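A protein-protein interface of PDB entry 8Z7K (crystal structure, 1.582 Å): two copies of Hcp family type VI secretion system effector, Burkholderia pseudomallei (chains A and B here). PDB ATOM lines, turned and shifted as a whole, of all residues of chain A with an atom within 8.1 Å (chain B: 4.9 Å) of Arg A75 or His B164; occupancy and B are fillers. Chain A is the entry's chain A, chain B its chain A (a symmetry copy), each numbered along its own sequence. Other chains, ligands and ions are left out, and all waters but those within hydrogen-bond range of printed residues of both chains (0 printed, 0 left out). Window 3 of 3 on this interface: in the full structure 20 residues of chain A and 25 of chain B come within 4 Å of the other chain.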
ATOM      1  N   ILE A  25       7.466  18.942  15.221  1.00  0.00           N
ATOM      2  CA  ILE A  25       6.838  18.464  13.994  1.00  0.00           C
ATOM      3  C   ILE A  25       6.645  16.954  14.149  1.00  0.00           C
ATOM      4  O   ILE A  25       7.643  16.244  14.280  1.00  0.00           O
ATOM      5  CB  ILE A  25       7.715  18.836  12.776  1.00  0.00           C
ATOM      6  CG1 ILE A  25       7.885  20.353  12.609  1.00  0.00           C
ATOM      7  CG2 ILE A  25       7.194  18.234  11.479  1.00  0.00           C
ATOM      8  CD1 ILE A  25       8.854  20.735  11.505  1.00  0.00           C
ATOM      9  N   LYS A  26       5.387  16.489  14.124  1.00  0.00           N
ATOM     10  CA  LYS A  26       5.033  15.076  14.314  1.00  0.00           C
ATOM     11  C   LYS A  26       4.175  14.561  13.148  1.00  0.00           C
ATOM     12  O   LYS A  26       3.569  15.352  12.438  1.00  0.00           O
ATOM     13  CB  LYS A  26       4.206  14.882  15.584  1.00  0.00           C
ATOM     14  CG  LYS A  26       4.551  15.683  16.834  1.00  0.00           C
ATOM     15  CD  LYS A  26       3.447  15.509  17.877  1.00  0.00           C
ATOM     16  CE  LYS A  26       2.254  16.395  17.608  1.00  0.00           C
ATOM     17  NZ  LYS A  26       0.974  15.858  18.083  1.00  0.00           N
ATOM     18  N   GLY A  27       4.117  13.229  12.966  1.00  0.00           N
ATOM     19  CA  GLY A  27       3.157  12.570  12.075  1.00  0.00           C
ATOM     20  C   GLY A  27       1.858  12.247  12.811  1.00  0.00           C
ATOM     21  O   GLY A  27       1.605  12.851  13.850  1.00  0.00           O
ATOM     22  N   SER A  28       1.061  11.292  12.292  1.00  0.00           N
ATOM     23  CA  SER A  28      -0.097  10.764  13.018  1.00  0.00           C
ATOM     24  C   SER A  28       0.312  10.274  14.414  1.00  0.00           C
ATOM     25  O   SER A  28       1.270   9.479  14.455  1.00  0.00           O
ATOM     26  CB  SER A  28      -0.772   9.610  12.317  1.00  0.00           C
ATOM     27  OG  SER A  28       0.176   8.599  12.009  1.00  0.00           O
ATOM     28  N   ILE A  38       8.647  10.610  13.637  1.00  0.00           N
ATOM     29  CA  ILE A  38       8.097  10.431  12.303  1.00  0.00           C
ATOM     30  C   ILE A  38       8.744   9.196  11.691  1.00  0.00           C
ATOM     31  O   ILE A  38       9.974   9.068  11.689  1.00  0.00           O
ATOM     32  CB  ILE A  38       8.318  11.693  11.445  1.00  0.00           C
ATOM     33  CG1 ILE A  38       7.794  12.926  12.143  1.00  0.00           C
ATOM     34  CG2 ILE A  38       7.710  11.534  10.044  1.00  0.00           C
ATOM     35  CD1 ILE A  38       7.918  14.235  11.367  1.00  0.00           C
ATOM     36  N   LYS A  71       9.385   9.828   2.862  1.00  0.00           N
ATOM     37  CA  LYS A  71       8.341   9.607   3.876  1.00  0.00           C
ATOM     38  C   LYS A  71       6.974   9.684   3.211  1.00  0.00           C
ATOM     39  O   LYS A  71       6.831  10.319   2.179  1.00  0.00           O
ATOM     40  CB  LYS A  71       8.335  10.544   5.095  1.00  0.00           C
ATOM     41  CG  LYS A  71       8.221  12.051   4.811  1.00  0.00           C
ATOM     42  CD  LYS A  71       8.176  12.928   6.057  1.00  0.00           C
ATOM     43  CE  LYS A  71       6.903  12.873   6.824  1.00  0.00           C
ATOM     44  NZ  LYS A  71       5.796  13.450   6.045  1.00  0.00           N
ATOM     45  N   GLU A  72       5.968   9.052   3.852  1.00  0.00           N
ATOM     46  CA  GLU A  72       4.593   9.235   3.422  1.00  0.00           C
ATOM     47  C   GLU A  72       4.184  10.673   3.733  1.00  0.00           C
ATOM     48  O   GLU A  72       4.563  11.223   4.775  1.00  0.00           O
ATOM     49  CB  GLU A  72       3.611   8.214   4.020  1.00  0.00           C
ATOM     50  CG  GLU A  72       2.321   8.125   3.198  1.00  0.00           C
ATOM     51  CD  GLU A  72       1.314   7.077   3.612  1.00  0.00           C
ATOM     52  OE1 GLU A  72       1.330   6.687   4.805  1.00  0.00           O
ATOM     53  OE2 GLU A  72       0.535   6.642   2.731  1.00  0.00           O
ATOM     54  N   MET A  73       3.465  11.321   2.798  1.00  0.00           N
ATOM     55  CA  MET A  73       2.900  12.629   3.054  1.00  0.00           C
ATOM     56  C   MET A  73       1.903  12.477   4.211  1.00  0.00           C
ATOM     57  O   MET A  73       1.210  11.472   4.266  1.00  0.00           O
ATOM     58  CB  MET A  73       2.245  13.209   1.801  1.00  0.00           C
ATOM     59  CG  MET A  73       3.233  13.670   0.754  1.00  0.00           C
ATOM     60  SD  MET A  73       2.418  14.513  -0.614  1.00  0.00           S
ATOM     61  CE  MET A  73       1.829  16.002   0.223  1.00  0.00           C
ATOM     62  N   ASP A  74       1.904  13.430   5.133  1.00  0.00           N
ATOM     63  CA  ASP A  74       1.132  13.338   6.366  1.00  0.00           C
ATOM     64  C   ASP A  74       0.981  14.744   6.931  1.00  0.00           C
ATOM     65  O   ASP A  74       1.158  15.719   6.210  1.00  0.00           O
ATOM     66  CB  ASP A  74       1.769  12.321   7.307  1.00  0.00           C
ATOM     67  CG  ASP A  74       3.099  12.737   7.917  1.00  0.00           C
ATOM     68  OD1 ASP A  74       3.592  13.812   7.560  1.00  0.00           O
ATOM     69  OD2 ASP A  74       3.618  12.003   8.788  1.00  0.00           O
ATOM     70  N   ARG A  75       0.618  14.853   8.221  1.00  0.00           N
ATOM     71  CA  ARG A  75       0.341  16.130   8.861  1.00  0.00           C
ATOM     72  C   ARG A  75       1.584  17.004   9.048  1.00  0.00           C
ATOM     73  O   ARG A  75       1.452  18.202   9.288  1.00  0.00           O
ATOM     74  CB  ARG A  75      -0.429  15.908  10.183  1.00  0.00           C
ATOM     75  CG  ARG A  75       0.131  14.989  11.262  1.00  0.00           C
ATOM     76  CD  ARG A  75      -0.995  14.564  12.272  1.00  0.00           C
ATOM     77  NE  ARG A  75      -1.994  13.611  11.731  1.00  0.00           N
ATOM     78  CZ  ARG A  75      -3.271  13.469  12.155  1.00  0.00           C
ATOM     79  NH1 ARG A  75      -4.157  12.811  11.418  1.00  0.00           N
ATOM     80  NH2 ARG A  75      -3.694  14.064  13.273  1.00  0.00           N
ATOM     81  N   SER A  76       2.777  16.412   8.988  1.00  0.00           N
ATOM     82  CA  SER A  76       4.031  17.139   9.052  1.00  0.00           C
ATOM     83  C   SER A  76       4.384  17.774   7.702  1.00  0.00           C
ATOM     84  O   SER A  76       5.192  18.711   7.698  1.00  0.00           O
ATOM     85  CB  SER A  76       5.159  16.270   9.509  1.00  0.00           C
ATOM     86  OG  SER A  76       5.430  15.193   8.640  1.00  0.00           O
ATOM     87  N   SER A  77       3.792  17.262   6.606  1.00  0.00           N
ATOM     88  CA  SER A  77       4.116  17.693   5.249  1.00  0.00           C
ATOM     89  C   SER A  77       3.943  19.202   5.085  1.00  0.00           C
ATOM     90  O   SER A  77       4.885  19.866   4.606  1.00  0.00           O
ATOM     91  CB  SER A  77       3.373  16.933   4.209  1.00  0.00           C
ATOM     92  OG  SER A  77       3.668  15.557   4.259  1.00  0.00           O
ATOM     93  N   PRO A  78       2.827  19.839   5.556  1.00  0.00           N
ATOM     94  CA  PRO A  78       2.709  21.296   5.498  1.00  0.00           C
ATOM     95  C   PRO A  78       3.790  22.023   6.272  1.00  0.00           C
ATOM     96  O   PRO A  78       4.235  23.062   5.784  1.00  0.00           O
ATOM     97  CB  PRO A  78       1.321  21.627   6.077  1.00  0.00           C
ATOM     98  CG  PRO A  78       0.587  20.299   5.979  1.00  0.00           C
ATOM     99  CD  PRO A  78       1.631  19.234   6.154  1.00  0.00           C
ATOM    100  N   GLN A  79       4.195  21.452   7.435  1.00  0.00           N
ATOM    101  CA  GLN A  79       5.188  22.071   8.308  1.00  0.00           C
ATOM    102  C   GLN A  79       6.580  22.143   7.667  1.00  0.00           C
ATOM    103  O   GLN A  79       7.205  23.209   7.729  1.00  0.00           O
ATOM    104  CB  GLN A  79       5.244  21.358   9.652  1.00  0.00           C
ATOM    105  CG  GLN A  79       3.991  21.598  10.480  1.00  0.00           C
ATOM    106  CD  GLN A  79       3.912  20.729  11.708  1.00  0.00           C
ATOM    107  OE1 GLN A  79       4.074  19.502  11.692  1.00  0.00           O
ATOM    108  NE2 GLN A  79       3.499  21.359  12.778  1.00  0.00           N
ATOM    109  N   PHE A  80       7.025  21.027   7.086  1.00  0.00           N
ATOM    110  CA  PHE A  80       8.258  20.970   6.324  1.00  0.00           C
ATOM    111  C   PHE A  80       8.195  21.886   5.104  1.00  0.00           C
ATOM    112  O   PHE A  80       9.141  22.647   4.856  1.00  0.00           O
ATOM    113  CB  PHE A  80       8.519  19.527   5.906  1.00  0.00           C
ATOM    114  CG  PHE A  80       8.927  18.578   7.021  1.00  0.00           C
ATOM    115  CD1 PHE A  80      10.027  18.856   7.827  1.00  0.00           C
ATOM    116  CD2 PHE A  80       8.191  17.430   7.258  1.00  0.00           C
ATOM    117  CE1 PHE A  80      10.423  17.952   8.807  1.00  0.00           C
ATOM    118  CE2 PHE A  80       8.585  16.517   8.244  1.00  0.00           C
ATOM    119  CZ  PHE A  80       9.699  16.775   9.016  1.00  0.00           C
ATOM    120  N   GLU A 151       6.830  12.008  -0.204  1.00  0.00           N
ATOM    121  CA  GLU A 151       7.729  13.148  -0.374  1.00  0.00           C
ATOM    122  C   GLU A 151       9.168  12.762  -0.062  1.00  0.00           C
ATOM    123  O   GLU A 151       9.446  11.891   0.776  1.00  0.00           O
ATOM    124  CB  GLU A 151       7.232  14.345   0.404  1.00  0.00           C
ATOM    125  CG  GLU A 151       7.198  14.170   1.921  1.00  0.00           C
ATOM    126  CD  GLU A 151       6.386  15.241   2.618  1.00  0.00           C
ATOM    127  OE1 GLU A 151       6.114  15.049   3.827  1.00  0.00           O
ATOM    128  OE2 GLU A 151       5.971  16.228   1.982  1.00  0.00           O
ATOM    129  N   LEU B 114      -7.790  14.780   1.965  1.00  0.00           N
ATOM    130  CA  LEU B 114      -6.513  14.572   2.589  1.00  0.00           C
ATOM    131  C   LEU B 114      -5.764  15.896   2.675  1.00  0.00           C
ATOM    132  O   LEU B 114      -5.290  16.245   3.736  1.00  0.00           O
ATOM    133  CB  LEU B 114      -5.765  13.521   1.757  1.00  0.00           C
ATOM    134  CG  LEU B 114      -4.489  12.945   2.375  1.00  0.00           C
ATOM    135  CD1 LEU B 114      -4.800  12.229   3.697  1.00  0.00           C
ATOM    136  CD2 LEU B 114      -3.740  12.027   1.364  1.00  0.00           C
ATOM    137  N   PHE B 115      -5.557  16.540   1.517  1.00  0.00           N
ATOM    138  CA  PHE B 115      -4.689  17.678   1.359  1.00  0.00           C
ATOM    139  C   PHE B 115      -5.370  18.713   0.448  1.00  0.00           C
ATOM    140  O   PHE B 115      -6.038  18.339  -0.534  1.00  0.00           O
ATOM    141  CB  PHE B 115      -3.330  17.336   0.725  1.00  0.00           C
ATOM    142  CG  PHE B 115      -2.363  16.591   1.628  1.00  0.00           C
ATOM    143  CD1 PHE B 115      -1.822  17.205   2.764  1.00  0.00           C
ATOM    144  CD2 PHE B 115      -2.009  15.270   1.347  1.00  0.00           C
ATOM    145  CE1 PHE B 115      -0.942  16.507   3.602  1.00  0.00           C
ATOM    146  CE2 PHE B 115      -1.145  14.588   2.185  1.00  0.00           C
ATOM    147  CZ  PHE B 115      -0.635  15.198   3.314  1.00  0.00           C
ATOM    148  N   LEU B 162      -0.253  24.606   1.829  1.00  0.00           N
ATOM    149  CA  LEU B 162      -0.632  23.195   1.904  1.00  0.00           C
ATOM    150  C   LEU B 162      -1.315  23.009   3.250  1.00  0.00           C
ATOM    151  O   LEU B 162      -0.779  23.447   4.250  1.00  0.00           O
ATOM    152  CB  LEU B 162       0.531  22.203   1.779  1.00  0.00           C
ATOM    153  CG  LEU B 162       0.244  20.698   1.888  1.00  0.00           C
ATOM    154  CD1 LEU B 162      -0.697  20.239   0.797  1.00  0.00           C
ATOM    155  CD2 LEU B 162       1.521  19.834   1.843  1.00  0.00           C
ATOM    156  N   GLU B 163      -2.455  22.312   3.266  1.00  0.00           N
ATOM    157  CA  GLU B 163      -3.247  22.104   4.469  1.00  0.00           C
ATOM    158  C   GLU B 163      -3.626  20.632   4.557  1.00  0.00           C
ATOM    159  O   GLU B 163      -4.234  20.143   3.608  1.00  0.00           O
ATOM    160  CB  GLU B 163      -4.483  22.990   4.334  1.00  0.00           C
ATOM    161  CG  GLU B 163      -5.629  22.551   5.234  1.00  0.00           C
ATOM    162  CD  GLU B 163      -5.369  22.994   6.649  1.00  0.00           C
ATOM    163  OE1 GLU B 163      -4.487  22.341   7.222  1.00  0.00           O
ATOM    164  OE2 GLU B 163      -5.985  23.948   7.148  1.00  0.00           O
ATOM    165  N   HIS B 164      -3.233  19.968   5.667  1.00  0.00           N
ATOM    166  CA  HIS B 164      -3.643  18.604   6.025  1.00  0.00           C
ATOM    167  C   HIS B 164      -5.048  18.687   6.619  1.00  0.00           C
ATOM    168  O   HIS B 164      -5.254  19.338   7.662  1.00  0.00           O
ATOM    169  CB  HIS B 164      -2.709  17.965   7.088  1.00  0.00           C
ATOM    170  CG  HIS B 164      -3.073  16.537   7.371  1.00  0.00           C
ATOM    171  ND1 HIS B 164      -3.776  16.105   8.478  1.00  0.00           N
ATOM    172  CD2 HIS B 164      -2.769  15.424   6.690  1.00  0.00           C
ATOM    173  CE1 HIS B 164      -3.903  14.794   8.451  1.00  0.00           C
ATOM    174  NE2 HIS B 164      -3.311  14.350   7.362  1.00  0.00           N
ATOM    175  N   ALA B 165      -6.032  18.080   5.916  1.00  0.00           N
ATOM    176  CA  ALA B 165      -7.436  18.346   6.200  1.00  0.00           C
ATOM    177  C   ALA B 165      -7.836  17.791   7.571  1.00  0.00           C
ATOM    178  O   ALA B 165      -8.350  18.557   8.374  1.00  0.00           O
ATOM    179  CB  ALA B 165      -8.328  17.783   5.105  1.00  0.00           C
ATOM    180  N   GLU B 166      -7.631  16.473   7.799  1.00  0.00           N
ATOM    181  CA  GLU B 166      -8.034  15.794   9.034  1.00  0.00           C
ATOM    182  C   GLU B 166      -7.544  16.594  10.265  1.00  0.00           C
ATOM    183  O   GLU B 166      -8.316  16.884  11.161  1.00  0.00           O
ATOM    184  CB  GLU B 166      -7.510  14.354   9.165  1.00  0.00           C
ATOM    185  N   SER B 167      -6.285  17.043  10.259  1.00  0.00           N
ATOM    186  CA  SER B 167      -5.626  17.662  11.399  1.00  0.00           C
ATOM    187  C   SER B 167      -5.801  19.177  11.410  1.00  0.00           C
ATOM    188  O   SER B 167      -5.713  19.774  12.488  1.00  0.00           O
ATOM    189  CB  SER B 167      -4.155  17.335  11.400  1.00  0.00           C
ATOM    190  OG  SER B 167      -3.492  18.079  10.381  1.00  0.00           O
ATOM    191  N   GLY B 168      -5.925  19.805  10.221  1.00  0.00           N
ATOM    192  CA  GLY B 168      -5.953  21.260  10.086  1.00  0.00           C
ATOM    193  C   GLY B 168      -4.569  21.914  10.098  1.00  0.00           C
ATOM    194  O   GLY B 168      -4.484  23.118   9.970  1.00  0.00           O
ATOM    195  N   ILE B 169      -3.478  21.137  10.191  1.00  0.00           N
ATOM    196  CA  ILE B 169      -2.134  21.720  10.178  1.00  0.00           C
ATOM    197  C   ILE B 169      -1.898  22.260   8.765  1.00  0.00           C
ATOM    198  O   ILE B 169      -2.190  21.554   7.804  1.00  0.00           O
ATOM    199  CB  ILE B 169      -1.076  20.685  10.578  1.00  0.00           C
ATOM    200  CG1 ILE B 169      -1.336  20.222  12.024  1.00  0.00           C
ATOM    201  CG2 ILE B 169       0.354  21.209  10.362  1.00  0.00           C
ATOM    202  CD1 ILE B 169      -0.416  19.186  12.535  1.00  0.00           C
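No position is printed for both chains.
Met A73 touches Phe B115.
O of Asp A74 touches CE1 of Phe B115, 3.4 Å away.
CD2 of His B164 touches C of Asp A74 (3.8 Å).
Arg A75 touches His B164 (NH1 to CE1, 3.6 Å).
OG of Ser B167 touches CB of Arg A75 (3.8 Å).
Arg A75 touches Ile B169.
Pro A78 touches Leu B162 (CB to O, 3.3 Å).
His B164 touches Pro A78.
O of Ile B169 touches CG of Pro A78 (3.6 Å).
Gln A79 touches Ile B169.
The backbone NH (N) of Asp A74 sits at hydrogen-bond distance from the side-chain hydroxyl (OG) of Ser A77 (2.9 Å).
The backbone NH (N) of His B164 lies within hydrogen-bond range of the backbone carbonyl oxygen (O) of Ile B169, at 2.9 Å.
The side-chain hydroxyl (OG) of Ser A76 sits at hydrogen-bond distance from the side-chain carboxylate (OD1) of Asp A74, at 2.5 Å.
N of Ile B169 lies close to OE1 of Glu B163.
The side-chain hydroxyl (OG) of Ser B167 sits at hydrogen-bond distance from a ring nitrogen (ND1) of His B164.
The side-chain hydroxyl (OG) of Ser B167 is in hydrogen-bond range of the backbone NH (N) of Ile B169.
Printed residues of chain B that touch a printed residue of chain A: Phe B115, Leu B162, His B164, Ser B167 and Ile B169.
Hydrophobic or aromatic side chains of chain B that line the printed part of chain A: Phe B115, Leu B162, His B164 and Ile B169.
Of the 16 printed residues of chain A, 5 touch a printed residue of chain B.
Hydrophobic or aromatic side chains of chain A within 4 Å of the printed part of chain B: Met A73 and Pro A78.
Among the printed residues, 10 pairs touch across the chains.
Among the printed residues, no Asp or Glu carboxylate lies within 4 Å of a Lys or Arg side-chain nitrogen of the other chain.
Printed residues of chain B within 4 Å of Met A73: Phe B115 (3.7 Å).
Of the printed residues of chain B, Asp A74 touches Phe B115 (3.4 Å) and His B164 (3.8 Å).
Of chain B, only His B164 (3.6 Å), Ser B167 (3.8 Å) and Ile B169 (3.4 Å) come within 4 Å of Arg A75.
Of the printed residues of chain B, Pro A78 touches Leu B162, His B164 and Ile B169.
Printed residues of chain B within 4 Å of Gln A79: Ile B169.
His B164 touches just these residues of chain A: Asp A74, Arg A75 and Pro A78.
No residue of chain A comes within 4 Å of Ala B165.
Printed residues of chain A within 4 Å of Ser B167: Arg A75.
The nearest residue of chain A that does not touch His B164 is Ser A76 (6.0 Å).
The nearest printed residue of chain B that does not touch Pro A78 is Glu B163 (4.5 Å).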
